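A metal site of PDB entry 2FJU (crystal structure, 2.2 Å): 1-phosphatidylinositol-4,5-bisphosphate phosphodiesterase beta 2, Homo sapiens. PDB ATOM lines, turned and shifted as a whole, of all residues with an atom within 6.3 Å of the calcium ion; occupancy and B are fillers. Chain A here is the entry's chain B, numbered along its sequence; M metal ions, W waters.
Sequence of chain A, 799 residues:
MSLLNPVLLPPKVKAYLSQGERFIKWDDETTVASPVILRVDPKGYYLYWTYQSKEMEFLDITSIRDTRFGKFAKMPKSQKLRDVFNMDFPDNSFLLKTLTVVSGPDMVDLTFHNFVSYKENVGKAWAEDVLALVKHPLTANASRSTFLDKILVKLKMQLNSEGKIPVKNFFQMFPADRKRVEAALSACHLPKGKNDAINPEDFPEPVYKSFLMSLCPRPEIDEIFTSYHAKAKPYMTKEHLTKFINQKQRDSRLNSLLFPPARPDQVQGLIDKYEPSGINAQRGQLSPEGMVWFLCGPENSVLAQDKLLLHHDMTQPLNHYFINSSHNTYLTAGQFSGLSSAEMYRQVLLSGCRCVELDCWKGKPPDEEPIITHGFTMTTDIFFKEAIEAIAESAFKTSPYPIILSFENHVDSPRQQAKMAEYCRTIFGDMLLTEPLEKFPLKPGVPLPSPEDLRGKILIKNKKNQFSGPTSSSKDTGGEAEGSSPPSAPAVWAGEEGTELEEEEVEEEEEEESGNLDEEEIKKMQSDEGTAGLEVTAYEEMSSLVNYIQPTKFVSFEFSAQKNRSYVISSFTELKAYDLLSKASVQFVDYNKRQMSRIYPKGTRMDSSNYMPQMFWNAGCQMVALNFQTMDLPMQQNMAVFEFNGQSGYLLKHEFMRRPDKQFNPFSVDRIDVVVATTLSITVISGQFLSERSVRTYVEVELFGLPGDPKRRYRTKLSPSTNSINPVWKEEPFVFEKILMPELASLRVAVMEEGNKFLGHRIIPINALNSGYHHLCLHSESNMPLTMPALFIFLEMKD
The side-chain carboxylate (OE2) of Glu 408 lies within hydrogen-bond range of the side-chain hydroxyl (OG1) of Thr 531, at 2.5 Å.
The side-chain carboxylate (OE2) of Glu 408 sits at hydrogen-bond distance from the backbone NH (N) of Ala 532, 3.4 Å away.
The backbone carbonyl oxygen of Leu 358 sits at hydrogen-bond distance from the backbone NH of Glu 408 (2.9 Å).
The side-chain carboxylate (OD2) of Asp 359 sits close to the side-chain hydroxyl (OH) of Tyr 330 (2.6 Å).
Four residues have an atom within 4 Å of the calcium ion: Asn 328, Glu 357, Asp 359 and Glu 408.
Along chain A the residues within 4 Å of the calcium ion span positions 328 to 408.
The calcium ion is bound by OD1 of Asn 328, OE1 of Glu 408, OE2 of Glu 357, water W2, OD1 of Asp 359, water W1 and OD2 of Asp 359.
The calcium ion has seven donor atoms within binding distance.
Water W2 lies within hydrogen-bond range of the side-chain hydroxyl of Thr 531 (2.8 Å) and the side-chain amide nitrogen of Asn 328 (3.4 Å).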
ATOM      1  N   HIS A 327      -2.600  16.878 -27.951  1.00  0.00           N
ATOM      2  CA  HIS A 327      -2.964  18.218 -27.485  1.00  0.00           C
ATOM      3  C   HIS A 327      -4.425  18.554 -27.832  1.00  0.00           C
ATOM      4  O   HIS A 327      -4.882  18.184 -28.908  1.00  0.00           O
ATOM      5  CB  HIS A 327      -2.027  19.261 -28.116  1.00  0.00           C
ATOM      6  CG  HIS A 327      -2.450  20.674 -27.865  1.00  0.00           C
ATOM      7  ND1 HIS A 327      -2.964  21.474 -28.859  1.00  0.00           N
ATOM      8  CD2 HIS A 327      -2.449  21.416 -26.733  1.00  0.00           C
ATOM      9  CE1 HIS A 327      -3.269  22.663 -28.350  1.00  0.00           C
ATOM     10  NE2 HIS A 327      -2.961  22.649 -27.057  1.00  0.00           N
ATOM     11  N   ASN A 328      -5.124  19.275 -26.951  1.00  0.00           N
ATOM     12  CA  ASN A 328      -6.528  19.663 -27.171  1.00  0.00           C
ATOM     13  C   ASN A 328      -7.226  18.554 -27.964  1.00  0.00           C
ATOM     14  O   ASN A 328      -7.806  18.794 -29.028  1.00  0.00           O
ATOM     15  CB  ASN A 328      -6.627  20.986 -27.937  1.00  0.00           C
ATOM     16  CG  ASN A 328      -6.497  22.181 -27.013  1.00  0.00           C
ATOM     17  OD1 ASN A 328      -6.442  22.021 -25.793  1.00  0.00           O
ATOM     18  ND2 ASN A 328      -6.469  23.395 -27.582  1.00  0.00           N
ATOM     19  N   TYR A 330      -9.969  16.931 -27.849  1.00  0.00           N
ATOM     20  CA  TYR A 330     -11.367  17.068 -28.249  1.00  0.00           C
ATOM     21  C   TYR A 330     -11.600  17.762 -29.605  1.00  0.00           C
ATOM     22  O   TYR A 330     -12.682  17.649 -30.182  1.00  0.00           O
ATOM     23  CB  TYR A 330     -12.143  17.821 -27.165  1.00  0.00           C
ATOM     24  CG  TYR A 330     -11.559  19.187 -26.852  1.00  0.00           C
ATOM     25  CD1 TYR A 330     -10.505  19.337 -25.943  1.00  0.00           C
ATOM     26  CD2 TYR A 330     -12.040  20.335 -27.486  1.00  0.00           C
ATOM     27  CE1 TYR A 330      -9.938  20.588 -25.691  1.00  0.00           C
ATOM     28  CE2 TYR A 330     -11.486  21.591 -27.231  1.00  0.00           C
ATOM     29  CZ  TYR A 330     -10.431  21.708 -26.339  1.00  0.00           C
ATOM     30  OH  TYR A 330      -9.882  22.954 -26.120  1.00  0.00           O
ATOM     31  N   GLU A 357      -5.981  15.412 -23.530  1.00  0.00           N
ATOM     32  CA  GLU A 357      -6.326  16.660 -22.856  1.00  0.00           C
ATOM     33  C   GLU A 357      -7.814  17.011 -22.868  1.00  0.00           C
ATOM     34  O   GLU A 357      -8.501  16.806 -23.863  1.00  0.00           O
ATOM     35  CB  GLU A 357      -5.519  17.787 -23.508  1.00  0.00           C
ATOM     36  CG  GLU A 357      -5.583  19.116 -22.782  1.00  0.00           C
ATOM     37  CD  GLU A 357      -4.605  20.125 -23.355  1.00  0.00           C
ATOM     38  OE1 GLU A 357      -3.828  19.766 -24.274  1.00  0.00           O
ATOM     39  OE2 GLU A 357      -4.618  21.285 -22.895  1.00  0.00           O
ATOM     40  N   LEU A 358      -8.278  17.554 -21.751  1.00  0.00           N
ATOM     41  CA  LEU A 358      -9.675  17.954 -21.590  1.00  0.00           C
ATOM     42  C   LEU A 358      -9.742  19.380 -21.039  1.00  0.00           C
ATOM     43  O   LEU A 358      -9.331  19.624 -19.912  1.00  0.00           O
ATOM     44  CB  LEU A 358     -10.401  17.021 -20.604  1.00  0.00           C
ATOM     45  CG  LEU A 358     -10.577  15.538 -20.937  1.00  0.00           C
ATOM     46  CD1 LEU A 358      -9.231  14.822 -20.891  1.00  0.00           C
ATOM     47  CD2 LEU A 358     -11.530  14.904 -19.922  1.00  0.00           C
ATOM     48  N   ASP A 359     -10.255  20.314 -21.846  1.00  0.00           N
ATOM     49  CA  ASP A 359     -10.419  21.701 -21.413  1.00  0.00           C
ATOM     50  C   ASP A 359     -11.827  21.778 -20.845  1.00  0.00           C
ATOM     51  O   ASP A 359     -12.802  21.743 -21.592  1.00  0.00           O
ATOM     52  CB  ASP A 359     -10.268  22.668 -22.596  1.00  0.00           C
ATOM     53  CG  ASP A 359      -8.835  22.810 -23.065  1.00  0.00           C
ATOM     54  OD1 ASP A 359      -7.962  22.064 -22.556  1.00  0.00           O
ATOM     55  OD2 ASP A 359      -8.575  23.653 -23.943  1.00  0.00           O
ATOM     56  N   HIS A 374     -12.785  24.726 -26.482  1.00  0.00           N
ATOM     57  CA  HIS A 374     -11.651  25.616 -26.449  1.00  0.00           C
ATOM     58  C   HIS A 374     -12.320  26.943 -26.109  1.00  0.00           C
ATOM     59  O   HIS A 374     -12.983  27.559 -26.946  1.00  0.00           O
ATOM     60  CB  HIS A 374     -10.988  25.678 -27.831  1.00  0.00           C
ATOM     61  CG  HIS A 374      -9.653  26.361 -27.838  1.00  0.00           C
ATOM     62  ND1 HIS A 374      -9.062  26.842 -26.688  1.00  0.00           N
ATOM     63  CD2 HIS A 374      -8.805  26.650 -28.854  1.00  0.00           C
ATOM     64  CE1 HIS A 374      -7.905  27.405 -26.999  1.00  0.00           C
ATOM     65  NE2 HIS A 374      -7.732  27.305 -28.302  1.00  0.00           N
ATOM     66  N   GLU A 408      -7.436  20.829 -18.056  1.00  0.00           N
ATOM     67  CA  GLU A 408      -7.184  22.260 -18.085  1.00  0.00           C
ATOM     68  C   GLU A 408      -8.511  22.730 -17.522  1.00  0.00           C
ATOM     69  O   GLU A 408      -9.478  22.927 -18.254  1.00  0.00           O
ATOM     70  CB  GLU A 408      -6.978  22.797 -19.496  1.00  0.00           C
ATOM     71  CG  GLU A 408      -6.642  24.276 -19.475  1.00  0.00           C
ATOM     72  CD  GLU A 408      -6.571  24.886 -20.849  1.00  0.00           C
ATOM     73  OE1 GLU A 408      -5.714  24.444 -21.642  1.00  0.00           O
ATOM     74  OE2 GLU A 408      -7.375  25.808 -21.138  1.00  0.00           O
ATOM     75  N   THR A 531      -5.569  29.550 -23.289  1.00  0.00           N
ATOM     76  CA  THR A 531      -6.424  29.336 -22.129  1.00  0.00           C
ATOM     77  C   THR A 531      -5.724  28.535 -21.036  1.00  0.00           C
ATOM     78  O   THR A 531      -6.110  28.600 -19.862  1.00  0.00           O
ATOM     79  CB  THR A 531      -7.741  28.598 -22.526  1.00  0.00           C
ATOM     80  OG1 THR A 531      -7.425  27.353 -23.165  1.00  0.00           O
ATOM     81  CG2 THR A 531      -8.550  29.460 -23.494  1.00  0.00           C
ATOM     82  N   ALA A 532      -4.679  27.800 -21.403  1.00  0.00           N
ATOM     83  CA  ALA A 532      -3.931  27.008 -20.437  1.00  0.00           C
ATOM     84  C   ALA A 532      -3.143  27.916 -19.495  1.00  0.00           C
ATOM     85  O   ALA A 532      -2.635  27.452 -18.474  1.00  0.00           O
ATOM     86  CB  ALA A 532      -2.980  26.050 -21.152  1.00  0.00           C
HETATM   87 CA    CA M   1      -5.958  23.191 -23.718  1.00  0.00          CA
HETATM   88  O   HOH W   1      -3.621  23.805 -24.675  1.00  0.00           O
HETATM   89  O   HOH W   2      -6.384  25.408 -24.858  1.00  0.00           O
